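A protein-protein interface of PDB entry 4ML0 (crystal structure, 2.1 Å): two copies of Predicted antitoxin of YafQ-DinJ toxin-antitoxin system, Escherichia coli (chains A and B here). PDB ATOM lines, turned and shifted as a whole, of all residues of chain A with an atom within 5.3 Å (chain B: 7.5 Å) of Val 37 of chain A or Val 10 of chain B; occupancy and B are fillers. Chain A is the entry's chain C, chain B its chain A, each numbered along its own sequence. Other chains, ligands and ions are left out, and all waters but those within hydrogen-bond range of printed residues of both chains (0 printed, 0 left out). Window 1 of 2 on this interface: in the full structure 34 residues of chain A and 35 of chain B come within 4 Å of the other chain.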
ATOM      1  N   VAL A  10       3.917 -14.644  14.318  1.00  0.00           N
ATOM      2  CA  VAL A  10       3.586 -13.747  15.413  1.00  0.00           C
ATOM      3  C   VAL A  10       3.969 -12.350  14.961  1.00  0.00           C
ATOM      4  O   VAL A  10       5.054 -12.154  14.407  1.00  0.00           O
ATOM      5  CB  VAL A  10       4.360 -14.113  16.690  1.00  0.00           C
ATOM      6  CG1 VAL A  10       4.389 -12.934  17.672  1.00  0.00           C
ATOM      7  CG2 VAL A  10       3.731 -15.328  17.342  1.00  0.00           C
ATOM      8  N   ARG A  11       3.081 -11.385  15.174  1.00  0.00           N
ATOM      9  CA  ARG A  11       3.352 -10.004  14.776  1.00  0.00           C
ATOM     10  C   ARG A  11       3.032  -9.097  15.953  1.00  0.00           C
ATOM     11  O   ARG A  11       1.900  -9.103  16.448  1.00  0.00           O
ATOM     12  CB  ARG A  11       2.493  -9.634  13.560  1.00  0.00           C
ATOM     13  CG  ARG A  11       2.495  -8.160  13.164  1.00  0.00           C
ATOM     14  CD  ARG A  11       1.491  -7.910  12.025  1.00  0.00           C
ATOM     15  NE  ARG A  11       1.618  -6.571  11.447  1.00  0.00           N
ATOM     16  CZ  ARG A  11       2.544  -6.238  10.555  1.00  0.00           C
ATOM     17  NH1 ARG A  11       3.418  -7.153  10.142  1.00  0.00           N
ATOM     18  NH2 ARG A  11       2.597  -4.999  10.080  1.00  0.00           N
ATOM     19  N   ALA A  12       4.026  -8.342  16.424  1.00  0.00           N
ATOM     20  CA  ALA A  12       3.832  -7.469  17.586  1.00  0.00           C
ATOM     21  C   ALA A  12       4.423  -6.080  17.364  1.00  0.00           C
ATOM     22  O   ALA A  12       5.600  -5.951  17.010  1.00  0.00           O
ATOM     23  CB  ALA A  12       4.442  -8.107  18.851  1.00  0.00           C
ATOM     24  N   ARG A  13       3.611  -5.045  17.573  1.00  0.00           N
ATOM     25  CA  ARG A  13       4.113  -3.670  17.584  1.00  0.00           C
ATOM     26  C   ARG A  13       4.979  -3.486  18.807  1.00  0.00           C
ATOM     27  O   ARG A  13       4.634  -3.965  19.894  1.00  0.00           O
ATOM     28  CB  ARG A  13       2.960  -2.671  17.673  1.00  0.00           C
ATOM     29  CG  ARG A  13       2.130  -2.559  16.412  1.00  0.00           C
ATOM     30  CD  ARG A  13       0.731  -2.029  16.701  1.00  0.00           C
ATOM     31  NE  ARG A  13       0.024  -1.664  15.473  1.00  0.00           N
ATOM     32  CZ  ARG A  13      -0.593  -2.530  14.669  1.00  0.00           C
ATOM     33  NH1 ARG A  13      -0.598  -3.832  14.952  1.00  0.00           N
ATOM     34  NH2 ARG A  13      -1.207  -2.090  13.576  1.00  0.00           N
ATOM     35  N   ILE A  14       6.089  -2.774  18.647  1.00  0.00           N
ATOM     36  CA  ILE A  14       6.982  -2.515  19.768  1.00  0.00           C
ATOM     37  C   ILE A  14       7.801  -1.249  19.514  1.00  0.00           C
ATOM     38  O   ILE A  14       8.018  -0.865  18.366  1.00  0.00           O
ATOM     39  CB  ILE A  14       7.925  -3.714  20.009  1.00  0.00           C
ATOM     40  CG1 ILE A  14       8.626  -3.590  21.361  1.00  0.00           C
ATOM     41  CG2 ILE A  14       8.947  -3.839  18.885  1.00  0.00           C
ATOM     42  CD1 ILE A  14       9.635  -4.696  21.616  1.00  0.00           C
ATOM     43  N   LYS A  19      13.280  -2.694  20.808  1.00  0.00           N
ATOM     44  CA  LYS A  19      13.590  -3.768  19.866  1.00  0.00           C
ATOM     45  C   LYS A  19      15.089  -3.840  19.609  1.00  0.00           C
ATOM     46  O   LYS A  19      15.680  -4.914  19.657  1.00  0.00           O
ATOM     47  CB  LYS A  19      12.835  -3.551  18.549  1.00  0.00           C
ATOM     48  CG  LYS A  19      13.000  -4.689  17.531  1.00  0.00           C
ATOM     49  CD  LYS A  19      12.517  -4.255  16.153  1.00  0.00           C
ATOM     50  CE  LYS A  19      12.513  -5.423  15.174  1.00  0.00           C
ATOM     51  NZ  LYS A  19      12.016  -4.999  13.828  1.00  0.00           N
ATOM     52  N   ILE A  33      15.450 -12.057  17.924  1.00  0.00           N
ATOM     53  CA  ILE A  33      14.214 -11.854  18.683  1.00  0.00           C
ATOM     54  C   ILE A  33      13.203 -12.963  18.361  1.00  0.00           C
ATOM     55  O   ILE A  33      12.471 -13.447  19.230  1.00  0.00           O
ATOM     56  CB  ILE A  33      13.598 -10.448  18.416  1.00  0.00           C
ATOM     57  CG1 ILE A  33      14.391  -9.367  19.169  1.00  0.00           C
ATOM     58  CG2 ILE A  33      12.108 -10.404  18.815  1.00  0.00           C
ATOM     59  CD1 ILE A  33      13.995  -7.922  18.787  1.00  0.00           C
ATOM     60  N   SER A  34      13.172 -13.392  17.108  1.00  0.00           N
ATOM     61  CA  SER A  34      12.189 -14.390  16.707  1.00  0.00           C
ATOM     62  C   SER A  34      12.473 -15.722  17.404  1.00  0.00           C
ATOM     63  O   SER A  34      11.534 -16.441  17.775  1.00  0.00           O
ATOM     64  CB  SER A  34      12.120 -14.530  15.174  1.00  0.00           C
ATOM     65  OG  SER A  34      13.286 -15.147  14.666  1.00  0.00           O
ATOM     66  N   ASP A  35      13.759 -16.039  17.604  1.00  0.00           N
ATOM     67  CA  ASP A  35      14.157 -17.205  18.417  1.00  0.00           C
ATOM     68  C   ASP A  35      13.592 -17.132  19.841  1.00  0.00           C
ATOM     69  O   ASP A  35      13.013 -18.094  20.357  1.00  0.00           O
ATOM     70  CB  ASP A  35      15.686 -17.290  18.541  1.00  0.00           C
ATOM     71  CG  ASP A  35      16.375 -17.665  17.233  1.00  0.00           C
ATOM     72  OD1 ASP A  35      15.752 -18.354  16.386  1.00  0.00           O
ATOM     73  OD2 ASP A  35      17.560 -17.275  17.074  1.00  0.00           O
ATOM     74  N   LEU A  36      13.787 -15.990  20.489  1.00  0.00           N
ATOM     75  CA  LEU A  36      13.269 -15.803  21.844  1.00  0.00           C
ATOM     76  C   LEU A  36      11.741 -15.896  21.883  1.00  0.00           C
ATOM     77  O   LEU A  36      11.158 -16.428  22.826  1.00  0.00           O
ATOM     78  CB  LEU A  36      13.743 -14.461  22.410  1.00  0.00           C
ATOM     79  CG  LEU A  36      13.251 -14.176  23.836  1.00  0.00           C
ATOM     80  CD1 LEU A  36      13.662 -15.314  24.756  1.00  0.00           C
ATOM     81  CD2 LEU A  36      13.808 -12.861  24.349  1.00  0.00           C
ATOM     82  N   VAL A  37      11.085 -15.376  20.856  1.00  0.00           N
ATOM     83  CA  VAL A  37       9.634 -15.445  20.791  1.00  0.00           C
ATOM     84  C   VAL A  37       9.172 -16.901  20.716  1.00  0.00           C
ATOM     85  O   VAL A  37       8.256 -17.305  21.445  1.00  0.00           O
ATOM     86  CB  VAL A  37       9.080 -14.633  19.579  1.00  0.00           C
ATOM     87  CG1 VAL A  37       7.603 -14.935  19.365  1.00  0.00           C
ATOM     88  CG2 VAL A  37       9.263 -13.141  19.819  1.00  0.00           C
ATOM     89  N   ARG A  38       9.794 -17.688  19.837  1.00  0.00           N
ATOM     90  CA  ARG A  38       9.425 -19.110  19.720  1.00  0.00           C
ATOM     91  C   ARG A  38       9.681 -19.871  21.022  1.00  0.00           C
ATOM     92  O   ARG A  38       8.841 -20.653  21.489  1.00  0.00           O
ATOM     93  CB  ARG A  38      10.188 -19.787  18.559  1.00  0.00           C
ATOM     94  CG  ARG A  38       9.537 -19.603  17.159  1.00  0.00           C
ATOM     95  CD  ARG A  38      10.363 -20.310  16.078  1.00  0.00           C
ATOM     96  NE  ARG A  38      11.679 -19.692  15.921  1.00  0.00           N
ATOM     97  CZ  ARG A  38      11.926 -18.679  15.096  1.00  0.00           C
ATOM     98  NH1 ARG A  38      10.943 -18.189  14.351  1.00  0.00           N
ATOM     99  NH2 ARG A  38      13.152 -18.168  15.002  1.00  0.00           N
ATOM    100  N   ILE A  39      10.858 -19.660  21.595  1.00  0.00           N
ATOM    101  CA  ILE A  39      11.217 -20.303  22.864  1.00  0.00           C
ATOM    102  C   ILE A  39      10.220 -19.966  23.985  1.00  0.00           C
ATOM    103  O   ILE A  39       9.732 -20.853  24.720  1.00  0.00           O
ATOM    104  CB  ILE A  39      12.652 -19.876  23.260  1.00  0.00           C
ATOM    105  CG1 ILE A  39      13.656 -20.493  22.280  1.00  0.00           C
ATOM    106  CG2 ILE A  39      12.992 -20.279  24.685  1.00  0.00           C
ATOM    107  CD1 ILE A  39      15.066 -19.903  22.381  1.00  0.00           C
ATOM    108  N   THR A  40       9.903 -18.677  24.116  1.00  0.00           N
ATOM    109  CA  THR A  40       9.003 -18.228  25.175  1.00  0.00           C
ATOM    110  C   THR A  40       7.568 -18.741  24.968  1.00  0.00           C
ATOM    111  O   THR A  40       6.921 -19.190  25.916  1.00  0.00           O
ATOM    112  CB  THR A  40       8.993 -16.689  25.270  1.00  0.00           C
ATOM    113  OG1 THR A  40      10.330 -16.236  25.486  1.00  0.00           O
ATOM    114  CG2 THR A  40       8.140 -16.220  26.438  1.00  0.00           C
ATOM    115  N   LEU A  41       7.064 -18.666  23.736  1.00  0.00           N
ATOM    116  CA  LEU A  41       5.711 -19.148  23.472  1.00  0.00           C
ATOM    117  C   LEU A  41       5.637 -20.664  23.677  1.00  0.00           C
ATOM    118  O   LEU A  41       4.636 -21.190  24.162  1.00  0.00           O
ATOM    119  CB  LEU A  41       5.251 -18.732  22.067  1.00  0.00           C
ATOM    120  CG  LEU A  41       4.982 -17.221  21.955  1.00  0.00           C
ATOM    121  CD1 LEU A  41       4.524 -16.831  20.564  1.00  0.00           C
ATOM    122  CD2 LEU A  41       3.944 -16.795  22.976  1.00  0.00           C
ATOM    123  N   THR A  42       6.714 -21.363  23.340  1.00  0.00           N
ATOM    124  CA  THR A  42       6.756 -22.810  23.576  1.00  0.00           C
ATOM    125  C   THR A  42       6.651 -23.117  25.072  1.00  0.00           C
ATOM    126  O   THR A  42       5.898 -24.006  25.477  1.00  0.00           O
ATOM    127  CB  THR A  42       8.047 -23.424  23.012  1.00  0.00           C
ATOM    128  OG1 THR A  42       8.038 -23.305  21.584  1.00  0.00           O
ATOM    129  CG2 THR A  42       8.163 -24.913  23.399  1.00  0.00           C
ATOM    130  N   ALA B   8       8.368  -0.092  15.791  1.00  0.00           N
ATOM    131  CA  ALA B   8       8.757  -1.173  14.897  1.00  0.00           C
ATOM    132  C   ALA B   8       7.853  -2.389  15.084  1.00  0.00           C
ATOM    133  O   ALA B   8       6.914  -2.363  15.883  1.00  0.00           O
ATOM    134  CB  ALA B   8      10.206  -1.546  15.132  1.00  0.00           C
ATOM    135  N   PHE B   9       8.140  -3.453  14.341  1.00  0.00           N
ATOM    136  CA  PHE B   9       7.400  -4.698  14.495  1.00  0.00           C
ATOM    137  C   PHE B   9       8.319  -5.865  14.787  1.00  0.00           C
ATOM    138  O   PHE B   9       9.399  -5.974  14.223  1.00  0.00           O
ATOM    139  CB  PHE B   9       6.583  -5.021  13.242  1.00  0.00           C
ATOM    140  CG  PHE B   9       5.366  -4.158  13.072  1.00  0.00           C
ATOM    141  CD1 PHE B   9       4.146  -4.557  13.593  1.00  0.00           C
ATOM    142  CD2 PHE B   9       5.442  -2.951  12.387  1.00  0.00           C
ATOM    143  CE1 PHE B   9       3.012  -3.770  13.429  1.00  0.00           C
ATOM    144  CE2 PHE B   9       4.313  -2.155  12.224  1.00  0.00           C
ATOM    145  CZ  PHE B   9       3.099  -2.561  12.749  1.00  0.00           C
ATOM    146  N   VAL B  10       7.870  -6.732  15.688  1.00  0.00           N
ATOM    147  CA  VAL B  10       8.454  -8.047  15.852  1.00  0.00           C
ATOM    148  C   VAL B  10       7.658  -8.965  14.939  1.00  0.00           C
ATOM    149  O   VAL B  10       6.422  -8.955  14.975  1.00  0.00           O
ATOM    150  CB  VAL B  10       8.308  -8.536  17.301  1.00  0.00           C
ATOM    151  CG1 VAL B  10       8.698 -10.000  17.408  1.00  0.00           C
ATOM    152  CG2 VAL B  10       9.159  -7.683  18.232  1.00  0.00           C
ATOM    153  N   ARG B  11       8.349  -9.740  14.105  1.00  0.00           N
ATOM    154  CA  ARG B  11       7.684 -10.672  13.203  1.00  0.00           C
ATOM    155  C   ARG B  11       8.407 -11.998  13.336  1.00  0.00           C
ATOM    156  O   ARG B  11       9.587 -12.087  13.006  1.00  0.00           O
ATOM    157  CB  ARG B  11       7.777 -10.184  11.742  1.00  0.00           C
ATOM    158  CG  ARG B  11       7.218  -8.788  11.482  1.00  0.00           C
ATOM    159  CD  ARG B  11       7.444  -8.369  10.020  1.00  0.00           C
ATOM    160  NE  ARG B  11       7.135  -6.957   9.794  1.00  0.00           N
ATOM    161  CZ  ARG B  11       8.016  -5.968   9.923  1.00  0.00           C
ATOM    162  NH1 ARG B  11       9.262  -6.241  10.276  1.00  0.00           N
ATOM    163  NH2 ARG B  11       7.654  -4.705   9.695  1.00  0.00           N
ATOM    164  N   ALA B  12       7.711 -13.031  13.806  1.00  0.00           N
ATOM    165  CA  ALA B  12       8.377 -14.298  14.082  1.00  0.00           C
ATOM    166  C   ALA B  12       7.604 -15.470  13.504  1.00  0.00           C
ATOM    167  O   ALA B  12       6.416 -15.656  13.791  1.00  0.00           O
ATOM    168  CB  ALA B  12       8.578 -14.489  15.600  1.00  0.00           C
ATOM    169  N   ARG B  13       8.282 -16.264  12.690  1.00  0.00           N
ATOM    170  CA  ARG B  13       7.679 -17.478  12.171  1.00  0.00           C
ATOM    171  C   ARG B  13       7.402 -18.428  13.338  1.00  0.00           C
ATOM    172  O   ARG B  13       8.192 -18.531  14.277  1.00  0.00           O
ATOM    173  CB  ARG B  13       8.580 -18.148  11.129  1.00  0.00           C
ATOM    174  CG  ARG B  13       8.022 -19.477  10.616  1.00  0.00           C
ATOM    175  CD  ARG B  13       8.921 -20.154   9.578  1.00  0.00           C
ATOM    176  NE  ARG B  13       8.426 -19.981   8.209  1.00  0.00           N
ATOM    177  CZ  ARG B  13       7.304 -20.520   7.736  1.00  0.00           C
ATOM    178  NH1 ARG B  13       6.528 -21.272   8.514  1.00  0.00           N
ATOM    179  NH2 ARG B  13       6.951 -20.302   6.476  1.00  0.00           N
ATOM    180  N   ILE B  14       6.259 -19.102  13.287  1.00  0.00           N
ATOM    181  CA  ILE B  14       5.882 -20.015  14.367  1.00  0.00           C
ATOM    182  C   ILE B  14       4.894 -21.079  13.894  1.00  0.00           C
ATOM    183  O   ILE B  14       4.118 -20.842  12.964  1.00  0.00           O
ATOM    184  CB  ILE B  14       5.291 -19.229  15.564  1.00  0.00           C
ATOM    185  CG1 ILE B  14       5.147 -20.123  16.793  1.00  0.00           C
ATOM    186  CG2 ILE B  14       3.946 -18.589  15.186  1.00  0.00           C
ATOM    187  CD1 ILE B  14       4.959 -19.335  18.068  1.00  0.00           C
ATOM    188  N   LEU B  18       0.953 -24.350  17.986  1.00  0.00           N
ATOM    189  CA  LEU B  18       1.653 -23.762  19.131  1.00  0.00           C
ATOM    190  C   LEU B  18       1.134 -22.343  19.387  1.00  0.00           C
ATOM    191  O   LEU B  18       0.765 -22.000  20.510  1.00  0.00           O
ATOM    192  CB  LEU B  18       3.163 -23.745  18.855  1.00  0.00           C
ATOM    193  CG  LEU B  18       4.107 -22.848  19.683  1.00  0.00           C
ATOM    194  CD1 LEU B  18       3.859 -23.024  21.157  1.00  0.00           C
ATOM    195  CD2 LEU B  18       5.552 -23.214  19.374  1.00  0.00           C
ATOM    196  N   ILE B  33      -0.666 -12.472  22.723  1.00  0.00           N
ATOM    197  CA  ILE B  33       0.703 -12.847  22.378  1.00  0.00           C
ATOM    198  C   ILE B  33       1.605 -11.616  22.262  1.00  0.00           C
ATOM    199  O   ILE B  33       2.745 -11.619  22.732  1.00  0.00           O
ATOM    200  CB  ILE B  33       0.755 -13.670  21.088  1.00  0.00           C
ATOM    201  CG1 ILE B  33       0.279 -15.102  21.368  1.00  0.00           C
ATOM    202  CG2 ILE B  33       2.180 -13.699  20.531  1.00  0.00           C
ATOM    203  CD1 ILE B  33       0.358 -16.007  20.167  1.00  0.00           C
ATOM    204  N   LEU B  36       2.792 -10.488  25.647  1.00  0.00           N
ATOM    205  CA  LEU B  36       3.887 -11.310  26.164  1.00  0.00           C
ATOM    206  C   LEU B  36       5.202 -10.974  25.461  1.00  0.00           C
ATOM    207  O   LEU B  36       6.261 -10.931  26.085  1.00  0.00           O
ATOM    208  CB  LEU B  36       3.553 -12.787  25.941  1.00  0.00           C
ATOM    209  CG  LEU B  36       4.143 -13.887  26.831  1.00  0.00           C
ATOM    210  CD1 LEU B  36       4.815 -14.890  25.949  1.00  0.00           C
ATOM    211  CD2 LEU B  36       5.098 -13.372  27.878  1.00  0.00           C
ATOM    212  N   VAL B  37       5.141 -10.742  24.152  1.00  0.00           N
ATOM    213  CA  VAL B  37       6.339 -10.345  23.420  1.00  0.00           C
ATOM    214  C   VAL B  37       6.922  -9.038  23.957  1.00  0.00           C
ATOM    215  O   VAL B  37       8.126  -8.951  24.260  1.00  0.00           O
ATOM    216  CB  VAL B  37       6.062 -10.233  21.906  1.00  0.00           C
ATOM    217  CG1 VAL B  37       7.258  -9.603  21.195  1.00  0.00           C
ATOM    218  CG2 VAL B  37       5.776 -11.637  21.322  1.00  0.00           C
ATOM    219  N   ARG B  38       6.079  -8.020  24.090  1.00  0.00           N
ATOM    220  CA  ARG B  38       6.573  -6.737  24.607  1.00  0.00           C
ATOM    221  C   ARG B  38       7.106  -6.836  26.038  1.00  0.00           C
ATOM    222  O   ARG B  38       8.158  -6.292  26.360  1.00  0.00           O
ATOM    223  CB  ARG B  38       5.484  -5.662  24.522  1.00  0.00           C
ATOM    224  CG  ARG B  38       5.335  -5.048  23.113  1.00  0.00           C
ATOM    225  CD  ARG B  38       4.223  -3.982  23.106  1.00  0.00           C
ATOM    226  NE  ARG B  38       2.915  -4.548  23.442  1.00  0.00           N
ATOM    227  CZ  ARG B  38       2.001  -4.906  22.541  1.00  0.00           C
ATOM    228  NH1 ARG B  38       2.247  -4.749  21.242  1.00  0.00           N
ATOM    229  NH2 ARG B  38       0.838  -5.418  22.939  1.00  0.00           N
ATOM    230  N   THR B  40       8.254  -9.480  27.618  1.00  0.00           N
ATOM    231  CA  THR B  40       9.487 -10.267  27.621  1.00  0.00           C
ATOM    232  C   THR B  40      10.672  -9.454  27.094  1.00  0.00           C
ATOM    233  O   THR B  40      11.746  -9.430  27.710  1.00  0.00           O
ATOM    234  CB  THR B  40       9.338 -11.570  26.776  1.00  0.00           C
ATOM    235  OG1 THR B  40       8.223 -12.340  27.255  1.00  0.00           O
ATOM    236  CG2 THR B  40      10.589 -12.399  26.872  1.00  0.00           C
ATOM    237  N   LEU B  41      10.492  -8.788  25.957  1.00  0.00           N
ATOM    238  CA  LEU B  41      11.601  -8.009  25.380  1.00  0.00           C
ATOM    239  C   LEU B  41      11.969  -6.835  26.283  1.00  0.00           C
ATOM    240  O   LEU B  41      13.136  -6.468  26.394  1.00  0.00           O
ATOM    241  CB  LEU B  41      11.274  -7.529  23.951  1.00  0.00           C
ATOM    242  CG  LEU B  41      11.090  -8.636  22.902  1.00  0.00           C
ATOM    243  CD1 LEU B  41      10.785  -8.053  21.534  1.00  0.00           C
ATOM    244  CD2 LEU B  41      12.332  -9.477  22.826  1.00  0.00           C
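Of the 14 printed residues of chain B, 14 touch a printed residue of chain A. Printed residues of chain B that touch a printed residue of chain A: Ala 8, Phe 9, Val 10, Arg 11, Ala 12, Arg 13, Ile 14, Leu 18, Ile 33, Leu 36, Val 37, Arg 38, Thr 40 and Leu 41. Hydrophobic or aromatic side chains of chain B that line the printed part of chain A: Ala 8, Phe 9, Val 10, Ala 12, Ile 14, Leu 18, Ile 33, Leu 36, Val 37 and Leu 41. Along chain B the printed residues that touch a printed residue of chain A span positions 8 to 41. Hydrophobic or aromatic side chains of chain A within 4 Å of the printed part of chain B: Val 10, Ala 12, Ile 14, Ile 33, Leu 36, Val 37 and Leu 41. Along chain A the printed residues that touch a printed residue of chain B span positions 10 to 42.
O of Leu 36 of chain A sits at hydrogen-bond distance from OG1 of Thr 40 of chain A (2.8 Å). The side-chain hydroxyl of Thr 40 of chain B is in hydrogen-bond range of the backbone carbonyl oxygen of Leu 36 of chain B (2.7 Å). The side-chain carboxylate (OD1) of Asp 35 of chain A is in salt-bridge range of the guanidinium group (NH2) of Arg 38 of chain A (3.0 Å). The backbone carbonyl oxygen (O) of Arg 38 of chain A is in hydrogen-bond range of the side-chain hydroxyl (OG1) of Thr 42 of chain A. NH2 of Arg 38 of chain A is in hydrogen-bond range of OG of Ser 34 of chain A (3.0 Å).
Printed residues of chain B within 4 Å of Val 37 of chain A: Val 10 (3.9998 Å) and Ala 12 (3.9 Å). Of the printed residues of chain A, Val 10 of chain B touches Val 10 (3.5 Å), Arg 11 (3.3 Å), Ala 12 (2.7 Å), Ile 14 (3.9 Å), Ile 33 (3.7 Å) and Val 37 (3.9998 Å). Of the printed residues of chain B, Ile 14 of chain A touches Ala 8, Val 10 and Leu 41. Of the printed residues of chain B, Val 10 of chain A touches Val 10 (3.5 Å), Arg 11 (3.3 Å), Ala 12 (2.7 Å), Ile 14 (3.9 Å) and Ile 33 (3.7 Å). Ile 39 of chain A touches none of the printed residues of chain B.
Arg 11 of chain A touches its own counterpart, Arg 11 of chain B. Ala 12 of chain A touches Val 37 of chain B, and with the chains exchanged Val 37 of chain A touches Ala 12 of chain B. Ile 33 of chain A touches Leu 41 of chain B, and with the chains exchanged Leu 41 of chain A touches Ile 33 of chain B. Thr 40 of chain B touches its own counterpart, Thr 40 of chain A.
Arg 11 of chain A touches Phe 9 of chain B (NH2 to CE1, 3.6 Å). Ala 12 of chain A touches Ala 8 of chain B (O to O, 3.98 Å). Ala 12 of chain A touches Val 37 of chain B (CB to CG1, 3.96 Å). Arg 13 of chain A touches Phe 9 of chain B (CG to CE1, 3.3 Å). Ile 14 of chain A touches Val 10 of chain B (CG2 to CG2, 3.9 Å). Ala 8 of chain B touches Lys 19 of chain A. Val 37 of chain A touches Val 10 of chain B (CG2 to CG1, 3.9998 Å). CD1 of Leu 36 of chain B touches CG2 of Thr 40 of chain A, at 3.6 Å. Ile 14 of chain B touches Leu 41 of chain A. Thr 42 of chain A touches Leu 18 of chain B.
The backbone carbonyl oxygen of Ala 12 of chain B sits at hydrogen-bond distance from the backbone NH of Val 10 of chain A (2.7 Å). N of Ala 8 of chain B sits at hydrogen-bond distance from O of Ile 14 of chain A, at 2.7 Å. The backbone carbonyl oxygen (O) of Ala 12 of chain A is in hydrogen-bond range of the backbone NH (N) of Val 10 of chain B, 2.7 Å away. The guanidinium group of Arg 38 of chain A is in hydrogen-bond range of the backbone carbonyl oxygen of Arg 13 of chain B (2.8 Å). The backbone carbonyl oxygen (O) of Arg 13 of chain A sits at hydrogen-bond distance from the guanidinium group (NH1) of Arg 38 of chain B, at 2.9 Å. O of Phe 9 of chain B lies within hydrogen-bond range of NZ of Lys 19 of chain A (2.8 Å).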
